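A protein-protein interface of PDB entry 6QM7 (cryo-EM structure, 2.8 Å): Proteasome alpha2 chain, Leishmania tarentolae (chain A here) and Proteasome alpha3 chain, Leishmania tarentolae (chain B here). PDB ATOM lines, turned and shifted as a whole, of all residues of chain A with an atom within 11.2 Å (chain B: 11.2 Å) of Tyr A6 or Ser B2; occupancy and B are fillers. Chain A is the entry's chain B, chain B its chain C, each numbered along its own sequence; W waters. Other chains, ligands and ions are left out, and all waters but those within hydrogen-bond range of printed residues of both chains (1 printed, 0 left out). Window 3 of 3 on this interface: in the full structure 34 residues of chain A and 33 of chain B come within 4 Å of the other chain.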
ATOM      1  N   GLU A   3      11.971  28.167 -24.364  1.00  0.00           N
ATOM      2  CA  GLU A   3      12.402  29.529 -23.890  1.00  0.00           C
ATOM      3  C   GLU A   3      13.911  29.535 -23.567  1.00  0.00           C
ATOM      4  O   GLU A   3      14.451  30.652 -23.374  1.00  0.00           O
ATOM      5  CB  GLU A   3      11.537  29.976 -22.698  1.00  0.00           C
ATOM      6  CG  GLU A   3      11.056  31.429 -22.758  1.00  0.00           C
ATOM      7  CD  GLU A   3      11.903  32.458 -22.021  1.00  0.00           C
ATOM      8  OE1 GLU A   3      12.785  33.066 -22.663  1.00  0.00           O
ATOM      9  OE2 GLU A   3      11.660  32.672 -20.814  1.00  0.00           O
ATOM     10  N   ALA A   4      14.569  28.366 -23.488  1.00  0.00           N
ATOM     11  CA  ALA A   4      16.046  28.231 -23.561  1.00  0.00           C
ATOM     12  C   ALA A   4      16.450  28.210 -25.038  1.00  0.00           C
ATOM     13  O   ALA A   4      15.932  27.351 -25.762  1.00  0.00           O
ATOM     14  CB  ALA A   4      16.517  26.990 -22.842  1.00  0.00           C
ATOM     15  N   PHE A   5      17.275  29.163 -25.477  1.00  0.00           N
ATOM     16  CA  PHE A   5      17.708  29.298 -26.892  1.00  0.00           C
ATOM     17  C   PHE A   5      19.226  29.182 -27.017  1.00  0.00           C
ATOM     18  O   PHE A   5      19.717  29.276 -28.156  1.00  0.00           O
ATOM     19  CB  PHE A   5      17.261  30.635 -27.487  1.00  0.00           C
ATOM     20  CG  PHE A   5      15.773  30.850 -27.561  1.00  0.00           C
ATOM     21  CD1 PHE A   5      15.027  30.283 -28.585  1.00  0.00           C
ATOM     22  CD2 PHE A   5      15.130  31.648 -26.624  1.00  0.00           C
ATOM     23  CE1 PHE A   5      13.657  30.496 -28.660  1.00  0.00           C
ATOM     24  CE2 PHE A   5      13.759  31.860 -26.699  1.00  0.00           C
ATOM     25  CZ  PHE A   5      13.025  31.284 -27.717  1.00  0.00           C
ATOM     26  N   TYR A   6      19.945  29.004 -25.910  1.00  0.00           N
ATOM     27  CA  TYR A   6      21.409  28.761 -25.928  1.00  0.00           C
ATOM     28  C   TYR A   6      21.666  27.299 -26.291  1.00  0.00           C
ATOM     29  O   TYR A   6      20.898  26.436 -25.861  1.00  0.00           O
ATOM     30  CB  TYR A   6      22.065  29.135 -24.602  1.00  0.00           C
ATOM     31  CG  TYR A   6      21.635  28.316 -23.417  1.00  0.00           C
ATOM     32  CD1 TYR A   6      22.229  27.098 -23.137  1.00  0.00           C
ATOM     33  CD2 TYR A   6      20.649  28.771 -22.558  1.00  0.00           C
ATOM     34  CE1 TYR A   6      21.853  26.348 -22.035  1.00  0.00           C
ATOM     35  CE2 TYR A   6      20.247  28.025 -21.464  1.00  0.00           C
ATOM     36  CZ  TYR A   6      20.857  26.812 -21.198  1.00  0.00           C
ATOM     37  OH  TYR A   6      20.471  26.059 -20.124  1.00  0.00           O
ATOM     38  N   GLY A   7      22.724  27.049 -27.058  1.00  0.00           N
ATOM     39  CA  GLY A   7      23.107  25.712 -27.536  1.00  0.00           C
ATOM     40  C   GLY A   7      23.664  24.845 -26.419  1.00  0.00           C
ATOM     41  O   GLY A   7      24.476  25.352 -25.603  1.00  0.00           O
ATOM     42  N   LEU A   8      23.236  23.579 -26.400  1.00  0.00           N
ATOM     43  CA  LEU A   8      23.620  22.535 -25.411  1.00  0.00           C
ATOM     44  C   LEU A   8      24.803  21.731 -25.948  1.00  0.00           C
ATOM     45  O   LEU A   8      25.543  21.168 -25.130  1.00  0.00           O
ATOM     46  CB  LEU A   8      22.419  21.615 -25.185  1.00  0.00           C
ATOM     47  CG  LEU A   8      21.402  22.002 -24.107  1.00  0.00           C
ATOM     48  CD1 LEU A   8      21.363  23.494 -23.818  1.00  0.00           C
ATOM     49  CD2 LEU A   8      20.018  21.504 -24.503  1.00  0.00           C
ATOM     50  N   THR A   9      24.923  21.641 -27.274  1.00  0.00           N
ATOM     51  CA  THR A   9      26.049  20.999 -27.998  1.00  0.00           C
ATOM     52  C   THR A   9      27.057  22.086 -28.369  1.00  0.00           C
ATOM     53  O   THR A   9      26.683  23.003 -29.111  1.00  0.00           O
ATOM     54  CB  THR A   9      25.567  20.250 -29.251  1.00  0.00           C
ATOM     55  OG1 THR A   9      24.366  19.518 -28.976  1.00  0.00           O
ATOM     56  CG2 THR A   9      26.622  19.303 -29.784  1.00  0.00           C
ATOM     57  N   THR A  10      28.272  21.993 -27.835  1.00  0.00           N
ATOM     58  CA  THR A  10      29.388  22.934 -28.095  1.00  0.00           C
ATOM     59  C   THR A  10      30.662  22.124 -28.345  1.00  0.00           C
ATOM     60  O   THR A  10      30.711  20.942 -27.941  1.00  0.00           O
ATOM     61  CB  THR A  10      29.557  23.921 -26.930  1.00  0.00           C
ATOM     62  OG1 THR A  10      30.230  23.307 -25.830  1.00  0.00           O
ATOM     63  CG2 THR A  10      28.236  24.471 -26.444  1.00  0.00           C
ATOM     64  N   GLN A  19      28.562  16.300 -26.739  1.00  0.00           N
ATOM     65  CA  GLN A  19      27.135  15.929 -26.532  1.00  0.00           C
ATOM     66  C   GLN A  19      26.670  14.972 -27.636  1.00  0.00           C
ATOM     67  O   GLN A  19      25.736  14.207 -27.366  1.00  0.00           O
ATOM     68  CB  GLN A  19      26.256  17.178 -26.416  1.00  0.00           C
ATOM     69  CG  GLN A  19      25.175  17.075 -25.342  1.00  0.00           C
ATOM     70  CD  GLN A  19      25.741  16.742 -23.986  1.00  0.00           C
ATOM     71  OE1 GLN A  19      26.726  17.321 -23.543  1.00  0.00           O
ATOM     72  NE2 GLN A  19      25.144  15.766 -23.333  1.00  0.00           N
ATOM     73  N   GLU A 118      20.149  19.474 -37.029  1.00  0.00           N
ATOM     74  CA  GLU A 118      19.415  20.570 -36.340  1.00  0.00           C
ATOM     75  C   GLU A 118      19.630  20.422 -34.832  1.00  0.00           C
ATOM     76  O   GLU A 118      20.119  21.368 -34.206  1.00  0.00           O
ATOM     77  CB  GLU A 118      17.916  20.557 -36.623  1.00  0.00           C
ATOM     78  CG  GLU A 118      17.504  21.338 -37.853  1.00  0.00           C
ATOM     79  CD  GLU A 118      15.995  21.361 -38.095  1.00  0.00           C
ATOM     80  OE1 GLU A 118      15.244  20.702 -37.319  1.00  0.00           O
ATOM     81  OE2 GLU A 118      15.563  22.031 -39.067  1.00  0.00           O
ATOM     82  N   PHE A 119      19.369  19.241 -34.291  1.00  0.00           N
ATOM     83  CA  PHE A 119      19.394  18.981 -32.835  1.00  0.00           C
ATOM     84  C   PHE A 119      20.827  18.912 -32.279  1.00  0.00           C
ATOM     85  O   PHE A 119      20.977  18.955 -31.039  1.00  0.00           O
ATOM     86  CB  PHE A 119      18.532  17.759 -32.551  1.00  0.00           C
ATOM     87  CG  PHE A 119      17.061  18.085 -32.565  1.00  0.00           C
ATOM     88  CD1 PHE A 119      16.354  18.226 -31.377  1.00  0.00           C
ATOM     89  CD2 PHE A 119      16.387  18.290 -33.759  1.00  0.00           C
ATOM     90  CE1 PHE A 119      15.002  18.537 -31.391  1.00  0.00           C
ATOM     91  CE2 PHE A 119      15.038  18.595 -33.771  1.00  0.00           C
ATOM     92  CZ  PHE A 119      14.348  18.728 -32.587  1.00  0.00           C
ATOM     93  N   THR A 120      21.854  18.864 -33.130  1.00  0.00           N
ATOM     94  CA  THR A 120      23.281  19.008 -32.727  1.00  0.00           C
ATOM     95  C   THR A 120      23.719  20.478 -32.710  1.00  0.00           C
ATOM     96  O   THR A 120      24.871  20.713 -32.317  1.00  0.00           O
ATOM     97  CB  THR A 120      24.223  18.247 -33.665  1.00  0.00           C
ATOM     98  OG1 THR A 120      24.238  18.888 -34.941  1.00  0.00           O
ATOM     99  CG2 THR A 120      23.845  16.791 -33.824  1.00  0.00           C
ATOM    100  N   GLN A 121      22.874  21.421 -33.148  1.00  0.00           N
ATOM    101  CA  GLN A 121      23.279  22.844 -33.305  1.00  0.00           C
ATOM    102  C   GLN A 121      22.235  23.793 -32.729  1.00  0.00           C
ATOM    103  O   GLN A 121      22.633  24.673 -31.971  1.00  0.00           O
ATOM    104  CB  GLN A 121      23.526  23.189 -34.773  1.00  0.00           C
ATOM    105  CG  GLN A 121      24.139  24.570 -34.975  1.00  0.00           C
ATOM    106  CD  GLN A 121      24.949  24.675 -36.242  1.00  0.00           C
ATOM    107  OE1 GLN A 121      25.873  25.485 -36.341  1.00  0.00           O
ATOM    108  NE2 GLN A 121      24.609  23.851 -37.220  1.00  0.00           N
ATOM    109  N   SER A 122      20.968  23.642 -33.105  1.00  0.00           N
ATOM    110  CA  SER A 122      19.835  24.486 -32.647  1.00  0.00           C
ATOM    111  C   SER A 122      19.856  24.619 -31.128  1.00  0.00           C
ATOM    112  O   SER A 122      20.313  23.692 -30.426  1.00  0.00           O
ATOM    113  CB  SER A 122      18.494  23.954 -33.116  1.00  0.00           C
ATOM    114  OG  SER A 122      18.299  24.210 -34.505  1.00  0.00           O
ATOM    115  N   GLY A 123      19.365  25.758 -30.658  1.00  0.00           N
ATOM    116  CA  GLY A 123      19.406  26.144 -29.241  1.00  0.00           C
ATOM    117  C   GLY A 123      18.401  25.380 -28.405  1.00  0.00           C
ATOM    118  O   GLY A 123      17.244  25.174 -28.848  1.00  0.00           O
ATOM    119  N   GLY A 124      18.843  24.996 -27.215  1.00  0.00           N
ATOM    120  CA  GLY A 124      17.984  24.507 -26.130  1.00  0.00           C
ATOM    121  C   GLY A 124      17.504  23.103 -26.390  1.00  0.00           C
ATOM    122  O   GLY A 124      16.577  22.686 -25.693  1.00  0.00           O
ATOM    123  N   VAL A 125      18.142  22.382 -27.310  1.00  0.00           N
ATOM    124  CA  VAL A 125      17.841  20.948 -27.541  1.00  0.00           C
ATOM    125  C   VAL A 125      19.134  20.143 -27.504  1.00  0.00           C
ATOM    126  O   VAL A 125      20.160  20.633 -28.015  1.00  0.00           O
ATOM    127  CB  VAL A 125      17.061  20.722 -28.846  1.00  0.00           C
ATOM    128  CG1 VAL A 125      15.735  21.462 -28.833  1.00  0.00           C
ATOM    129  CG2 VAL A 125      17.865  21.082 -30.080  1.00  0.00           C
ATOM    130  N   ARG A 126      19.064  18.948 -26.921  1.00  0.00           N
ATOM    131  CA  ARG A 126      20.137  17.932 -27.032  1.00  0.00           C
ATOM    132  C   ARG A 126      19.947  17.156 -28.328  1.00  0.00           C
ATOM    133  O   ARG A 126      18.854  17.167 -28.896  1.00  0.00           O
ATOM    134  CB  ARG A 126      20.134  16.953 -25.858  1.00  0.00           C
ATOM    135  CG  ARG A 126      18.762  16.421 -25.491  1.00  0.00           C
ATOM    136  CD  ARG A 126      18.821  15.055 -24.852  1.00  0.00           C
ATOM    137  NE  ARG A 126      18.207  14.126 -25.790  1.00  0.00           N
ATOM    138  CZ  ARG A 126      17.032  13.533 -25.633  1.00  0.00           C
ATOM    139  NH1 ARG A 126      16.307  13.715 -24.545  1.00  0.00           N
ATOM    140  NH2 ARG A 126      16.580  12.739 -26.574  1.00  0.00           N
ATOM    141  N   PRO A 127      20.990  16.439 -28.808  1.00  0.00           N
ATOM    142  CA  PRO A 127      20.853  15.565 -29.967  1.00  0.00           C
ATOM    143  C   PRO A 127      19.962  14.342 -29.704  1.00  0.00           C
ATOM    144  O   PRO A 127      19.622  14.047 -28.559  1.00  0.00           O
ATOM    145  CB  PRO A 127      22.283  15.080 -30.229  1.00  0.00           C
ATOM    146  CG  PRO A 127      23.162  16.039 -29.475  1.00  0.00           C
ATOM    147  CD  PRO A 127      22.354  16.402 -28.252  1.00  0.00           C
ATOM    148  N   SER B   2      18.310  28.182 -15.994  1.00  0.00           N
ATOM    149  CA  SER B   2      18.723  27.822 -17.387  1.00  0.00           C
ATOM    150  C   SER B   2      19.856  28.749 -17.862  1.00  0.00           C
ATOM    151  O   SER B   2      20.756  28.232 -18.532  1.00  0.00           O
ATOM    152  CB  SER B   2      17.541  27.808 -18.350  1.00  0.00           C
ATOM    153  OG  SER B   2      17.634  26.758 -19.307  1.00  0.00           O
ATOM    154  N   HIS B   3      19.869  30.039 -17.503  1.00  0.00           N
ATOM    155  CA  HIS B   3      20.990  30.965 -17.839  1.00  0.00           C
ATOM    156  C   HIS B   3      22.297  30.427 -17.237  1.00  0.00           C
ATOM    157  O   HIS B   3      23.355  30.695 -17.815  1.00  0.00           O
ATOM    158  CB  HIS B   3      20.693  32.422 -17.421  1.00  0.00           C
ATOM    159  CG  HIS B   3      21.035  32.757 -16.002  1.00  0.00           C
ATOM    160  ND1 HIS B   3      20.118  32.644 -14.967  1.00  0.00           N
ATOM    161  CD2 HIS B   3      22.180  33.209 -15.439  1.00  0.00           C
ATOM    162  CE1 HIS B   3      20.685  33.002 -13.831  1.00  0.00           C
ATOM    163  NE2 HIS B   3      21.954  33.352 -14.094  1.00  0.00           N
ATOM    164  N   ARG B   4      22.210  29.696 -16.120  1.00  0.00           N
ATOM    165  CA  ARG B   4      23.354  29.094 -15.375  1.00  0.00           C
ATOM    166  C   ARG B   4      24.156  28.165 -16.291  1.00  0.00           C
ATOM    167  O   ARG B   4      25.385  28.129 -16.148  1.00  0.00           O
ATOM    168  CB  ARG B   4      22.858  28.300 -14.158  1.00  0.00           C
ATOM    169  CG  ARG B   4      22.146  29.129 -13.090  1.00  0.00           C
ATOM    170  CD  ARG B   4      21.800  28.362 -11.816  1.00  0.00           C
ATOM    171  NE  ARG B   4      22.988  27.749 -11.211  1.00  0.00           N
ATOM    172  CZ  ARG B   4      23.233  26.438 -11.063  1.00  0.00           C
ATOM    173  NH1 ARG B   4      24.370  26.048 -10.507  1.00  0.00           N
ATOM    174  NH2 ARG B   4      22.360  25.516 -11.444  1.00  0.00           N
ATOM    175  N   TYR B   5      23.475  27.446 -17.187  1.00  0.00           N
ATOM    176  CA  TYR B   5      24.031  26.341 -18.013  1.00  0.00           C
ATOM    177  C   TYR B   5      24.316  26.810 -19.448  1.00  0.00           C
ATOM    178  O   TYR B   5      24.586  25.948 -20.316  1.00  0.00           O
ATOM    179  CB  TYR B   5      23.073  25.145 -18.022  1.00  0.00           C
ATOM    180  CG  TYR B   5      22.487  24.780 -16.678  1.00  0.00           C
ATOM    181  CD1 TYR B   5      23.286  24.279 -15.658  1.00  0.00           C
ATOM    182  CD2 TYR B   5      21.131  24.947 -16.422  1.00  0.00           C
ATOM    183  CE1 TYR B   5      22.750  23.955 -14.422  1.00  0.00           C
ATOM    184  CE2 TYR B   5      20.580  24.626 -15.192  1.00  0.00           C
ATOM    185  CZ  TYR B   5      21.392  24.124 -14.190  1.00  0.00           C
ATOM    186  OH  TYR B   5      20.852  23.812 -12.976  1.00  0.00           O
ATOM    187  N   ASP B   6      24.266  28.122 -19.699  1.00  0.00           N
ATOM    188  CA  ASP B   6      24.680  28.733 -20.986  1.00  0.00           C
ATOM    189  C   ASP B   6      26.204  28.636 -21.078  1.00  0.00           C
ATOM    190  O   ASP B   6      26.894  29.074 -20.137  1.00  0.00           O
ATOM    191  CB  ASP B   6      24.185  30.176 -21.105  1.00  0.00           C
ATOM    192  CG  ASP B   6      24.223  30.774 -22.502  1.00  0.00           C
ATOM    193  OD1 ASP B   6      24.901  30.203 -23.383  1.00  0.00           O
ATOM    194  OD2 ASP B   6      23.576  31.817 -22.695  1.00  0.00           O
ATOM    195  N   SER B   7      26.685  28.071 -22.186  1.00  0.00           N
ATOM    196  CA  SER B   7      28.116  27.889 -22.547  1.00  0.00           C
ATOM    197  C   SER B   7      28.737  29.214 -23.008  1.00  0.00           C
ATOM    198  O   SER B   7      29.980  29.324 -22.970  1.00  0.00           O
ATOM    199  CB  SER B   7      28.211  26.854 -23.623  1.00  0.00           C
ATOM    200  OG  SER B   7      27.109  26.994 -24.514  1.00  0.00           O
ATOM    201  N   ARG B   8      27.895  30.154 -23.463  1.00  0.00           N
ATOM    202  CA  ARG B   8      28.273  31.499 -23.970  1.00  0.00           C
ATOM    203  C   ARG B   8      29.231  31.301 -25.150  1.00  0.00           C
ATOM    204  O   ARG B   8      30.430  31.605 -25.021  1.00  0.00           O
ATOM    205  CB  ARG B   8      28.802  32.359 -22.812  1.00  0.00           C
ATOM    206  CG  ARG B   8      27.752  33.245 -22.142  1.00  0.00           C
ATOM    207  CD  ARG B   8      27.683  33.107 -20.627  1.00  0.00           C
ATOM    208  NE  ARG B   8      29.000  32.958 -20.007  1.00  0.00           N
ATOM    209  CZ  ARG B   8      29.273  32.272 -18.891  1.00  0.00           C
ATOM    210  NH1 ARG B   8      28.322  31.640 -18.218  1.00  0.00           N
ATOM    211  NH2 ARG B   8      30.522  32.218 -18.452  1.00  0.00           N
ATOM    212  N   THR B   9      28.694  30.768 -26.250  1.00  0.00           N
ATOM    213  CA  THR B   9      29.445  30.385 -27.473  1.00  0.00           C
ATOM    214  C   THR B   9      29.933  31.664 -28.150  1.00  0.00           C
ATOM    215  O   THR B   9      31.131  31.734 -28.467  1.00  0.00           O
ATOM    216  CB  THR B   9      28.605  29.507 -28.422  1.00  0.00           C
ATOM    217  OG1 THR B   9      27.444  30.191 -28.897  1.00  0.00           O
ATOM    218  CG2 THR B   9      28.138  28.219 -27.781  1.00  0.00           C
ATOM    219  N   THR B  10      29.029  32.632 -28.334  1.00  0.00           N
ATOM    220  CA  THR B  10      29.237  33.888 -29.108  1.00  0.00           C
ATOM    221  C   THR B  10      29.698  34.996 -28.156  1.00  0.00           C
ATOM    222  O   THR B  10      29.031  36.051 -28.088  1.00  0.00           O
ATOM    223  CB  THR B  10      27.961  34.290 -29.863  1.00  0.00           C
ATOM    224  OG1 THR B  10      26.925  34.645 -28.942  1.00  0.00           O
ATOM    225  CG2 THR B  10      27.459  33.188 -30.770  1.00  0.00           C
ATOM    226  N   THR B  11      30.770  34.737 -27.413  1.00  0.00           N
ATOM    227  CA  THR B  11      31.430  35.718 -26.530  1.00  0.00           C
ATOM    228  C   THR B  11      32.919  35.706 -26.837  1.00  0.00           C
ATOM    229  O   THR B  11      33.441  34.649 -27.199  1.00  0.00           O
ATOM    230  CB  THR B  11      31.238  35.405 -25.041  1.00  0.00           C
ATOM    231  OG1 THR B  11      31.757  34.094 -24.822  1.00  0.00           O
ATOM    232  CG2 THR B  11      29.796  35.506 -24.600  1.00  0.00           C
ATOM    233  N   GLN B  20      34.931  29.030 -29.252  1.00  0.00           N
ATOM    234  CA  GLN B  20      34.083  28.032 -29.947  1.00  0.00           C
ATOM    235  C   GLN B  20      34.573  27.907 -31.393  1.00  0.00           C
ATOM    236  O   GLN B  20      34.507  26.788 -31.927  1.00  0.00           O
ATOM    237  CB  GLN B  20      32.598  28.380 -29.798  1.00  0.00           C
ATOM    238  CG  GLN B  20      31.707  27.197 -29.411  1.00  0.00           C
ATOM    239  CD  GLN B  20      32.237  26.418 -28.236  1.00  0.00           C
ATOM    240  OE1 GLN B  20      32.255  25.193 -28.247  1.00  0.00           O
ATOM    241  NE2 GLN B  20      32.717  27.129 -27.227  1.00  0.00           N
ATOM    242  N   TYR B 127      27.030  32.755 -36.846  1.00  0.00           N
ATOM    243  CA  TYR B 127      26.971  31.758 -35.750  1.00  0.00           C
ATOM    244  C   TYR B 127      28.119  31.978 -34.754  1.00  0.00           C
ATOM    245  O   TYR B 127      28.082  31.346 -33.693  1.00  0.00           O
ATOM    246  CB  TYR B 127      26.896  30.351 -36.350  1.00  0.00           C
ATOM    247  CG  TYR B 127      25.515  29.960 -36.821  1.00  0.00           C
ATOM    248  CD1 TYR B 127      24.817  28.923 -36.215  1.00  0.00           C
ATOM    249  CD2 TYR B 127      24.885  30.641 -37.853  1.00  0.00           C
ATOM    250  CE1 TYR B 127      23.543  28.561 -36.631  1.00  0.00           C
ATOM    251  CE2 TYR B 127      23.616  30.293 -38.285  1.00  0.00           C
ATOM    252  CZ  TYR B 127      22.938  29.249 -37.673  1.00  0.00           C
ATOM    253  OH  TYR B 127      21.685  28.900 -38.093  1.00  0.00           O
ATOM    254  N   TYR B 130      25.921  36.038 -33.261  1.00  0.00           N
ATOM    255  CA  TYR B 130      24.507  35.968 -32.812  1.00  0.00           C
ATOM    256  C   TYR B 130      24.168  34.530 -32.421  1.00  0.00           C
ATOM    257  O   TYR B 130      24.821  33.607 -32.916  1.00  0.00           O
ATOM    258  CB  TYR B 130      23.584  36.471 -33.928  1.00  0.00           C
ATOM    259  CG  TYR B 130      23.916  37.869 -34.389  1.00  0.00           C
ATOM    260  CD1 TYR B 130      24.894  38.099 -35.347  1.00  0.00           C
ATOM    261  CD2 TYR B 130      23.297  38.977 -33.822  1.00  0.00           C
ATOM    262  CE1 TYR B 130      25.238  39.387 -35.739  1.00  0.00           C
ATOM    263  CE2 TYR B 130      23.621  40.272 -34.209  1.00  0.00           C
ATOM    264  CZ  TYR B 130      24.601  40.478 -35.167  1.00  0.00           C
ATOM    265  OH  TYR B 130      24.927  41.749 -35.546  1.00  0.00           O
ATOM    266  N   GLY B 131      23.178  34.355 -31.539  1.00  0.00           N
ATOM    267  CA  GLY B 131      22.304  33.161 -31.506  1.00  0.00           C
ATOM    268  C   GLY B 131      22.666  32.137 -30.442  1.00  0.00           C
ATOM    269  O   GLY B 131      21.888  31.177 -30.293  1.00  0.00           O
ATOM    270  N   GLY B 132      23.806  32.304 -29.764  1.00  0.00           N
ATOM    271  CA  GLY B 132      24.212  31.499 -28.598  1.00  0.00           C
ATOM    272  C   GLY B 132      24.307  30.009 -28.875  1.00  0.00           C
ATOM    273  O   GLY B 132      24.199  29.226 -27.908  1.00  0.00           O
ATOM    274  N   VAL B 133      24.568  29.628 -30.123  1.00  0.00           N
ATOM    275  CA  VAL B 133      24.766  28.211 -30.555  1.00  0.00           C
ATOM    276  C   VAL B 133      26.197  28.080 -31.059  1.00  0.00           C
ATOM    277  O   VAL B 133      26.816  29.116 -31.319  1.00  0.00           O
ATOM    278  CB  VAL B 133      23.752  27.783 -31.627  1.00  0.00           C
ATOM    279  CG1 VAL B 133      22.372  27.641 -31.021  1.00  0.00           C
ATOM    280  CG2 VAL B 133      23.707  28.732 -32.817  1.00  0.00           C
ATOM    281  N   ARG B 134      26.689  26.851 -31.181  1.00  0.00           N
ATOM    282  CA  ARG B 134      28.058  26.578 -31.684  1.00  0.00           C
ATOM    283  C   ARG B 134      28.160  27.096 -33.111  1.00  0.00           C
ATOM    284  O   ARG B 134      27.155  27.145 -33.820  1.00  0.00           O
ATOM    285  CB  ARG B 134      28.398  25.085 -31.629  1.00  0.00           C
ATOM    286  CG  ARG B 134      27.522  24.189 -32.497  1.00  0.00           C
ATOM    287  CD  ARG B 134      27.951  22.745 -32.330  1.00  0.00           C
ATOM    288  NE  ARG B 134      27.260  21.844 -33.235  1.00  0.00           N
ATOM    289  CZ  ARG B 134      27.536  21.693 -34.526  1.00  0.00           C
ATOM    290  NH1 ARG B 134      28.497  22.405 -35.100  1.00  0.00           N
ATOM    291  NH2 ARG B 134      26.821  20.839 -35.243  1.00  0.00           N
ATOM    292  N   PRO B 135      29.370  27.459 -33.583  1.00  0.00           N
ATOM    293  CA  PRO B 135      29.608  27.656 -35.012  1.00  0.00           C
ATOM    294  C   PRO B 135      29.559  26.356 -35.830  1.00  0.00           C
ATOM    295  O   PRO B 135      29.596  25.283 -35.270  1.00  0.00           O
ATOM    296  CB  PRO B 135      31.031  28.230 -35.044  1.00  0.00           C
ATOM    297  CG  PRO B 135      31.686  27.659 -33.802  1.00  0.00           C
ATOM    298  CD  PRO B 135      30.578  27.682 -32.772  1.00  0.00           C
HETATM  299  O   HOH W   1      24.821  24.783 -30.139  1.00  0.00           O
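N of Gly A7 lies within hydrogen-bond range of O of Gly B132, at 2.8 Å. O of Thr A120 lies within hydrogen-bond range of NE of Arg B134, 2.8 Å away. The backbone carbonyl oxygen of Arg B134 lies close to the side-chain amide oxygen of Gln A121, 3.3 Å away. O of Gly A7 is in hydrogen-bond range of OG of Ser B7, 3.3 Å away. O of Ser B2 sits at hydrogen-bond distance from OH of Tyr A6 (2.7 Å).
N of Arg B8 lies within hydrogen-bond range of OD1 of Asp B6. O of Val B133 lies within hydrogen-bond range of OG1 of Thr B9 (2.7 Å). The backbone carbonyl oxygen (O) of Glu A118 lies close to the side-chain hydroxyl (OG) of Ser A122 (3.4 Å). The side-chain hydroxyl (OH) of Tyr B5 is in hydrogen-bond range of the guanidinium group (NH2) of Arg B4 (2.7 Å). O of Tyr A6 is in hydrogen-bond range of N of Gly A124, at 2.9 Å.
Ser B2 touches Ala A4. Phe A5 touches Gly B131 (O to O, 3.6 Å). Tyr A6 touches Tyr B5. OD1 of Asp B6 touches CB of Tyr A6, 3.3 Å away. Arg B134 touches Thr A9 (CD to O, 3.5 Å). CG2 of Thr A10 touches CG2 of Thr B9 (3.98 Å). Gln A121 touches Tyr B127 (OE1 to CD1, 3.6 Å). Gln A121 touches Val B133. Val B133 touches Ser A122. CG1 of Val B133 touches N of Gly A123, 3.6 Å away.
Ala A4 touches just one residue of chain B: Ser B2 (3.7 Å). Printed residues of chain B within 4 Å of Tyr A6: Ser B2 (2.7 Å), Tyr B5 (3.3 Å), Asp B6 (3.3 Å) and Gly B132 (3.5 Å). Of chain B, only Ser B7 (3.3 Å) and Gly B132 (2.8 Å) come within 4 Å of Gly A7. No residue of chain B comes within 4 Å of Leu A8. Printed residues of chain B within 4 Å of Thr A10: Ser B7, Thr B9 and Gln B20. Phe A119 touches none of the printed residues of chain B. Of chain B, only Val B133 (3.6 Å) comes within 4 Å of Gly A123. No residue of chain B comes within 4 Å of Gly A124. Ser B2 touches just these residues of chain A: Ala A4 and Tyr A6. Tyr B5 touches just one residue of chain A: Tyr A6 (3.3 Å). Printed residues of chain A within 4 Å of Ser B7: Gly A7 (3.3 Å) and Thr A10 (3.4 Å).
Hydrophobic or aromatic side chains of chain B that line the printed part of chain A: Tyr B5, Tyr B127 and Val B133. Of the 19 printed residues of chain A, 10 touch a printed residue of chain B. Printed residues of chain A that touch a printed residue of chain B: Ala A4, Phe A5, Tyr A6, Gly A7, Thr A9, Thr A10, Thr A120, Gln A121, Ser A122 and Gly A123. Among the printed residues, 19 pairs touch across the chains. Among the printed residues, no Asp or Glu carboxylate lies within 4 Å of a Lys or Arg side-chain nitrogen of the other chain.
Water W1 lies within hydrogen-bond range of the backbone carbonyl oxygen (O) of Thr A9 (2.8 Å), the backbone carbonyl oxygen (O) of Gln A121 (2.9 Å) and the backbone NH (N) of Arg B134 (3.0 Å).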
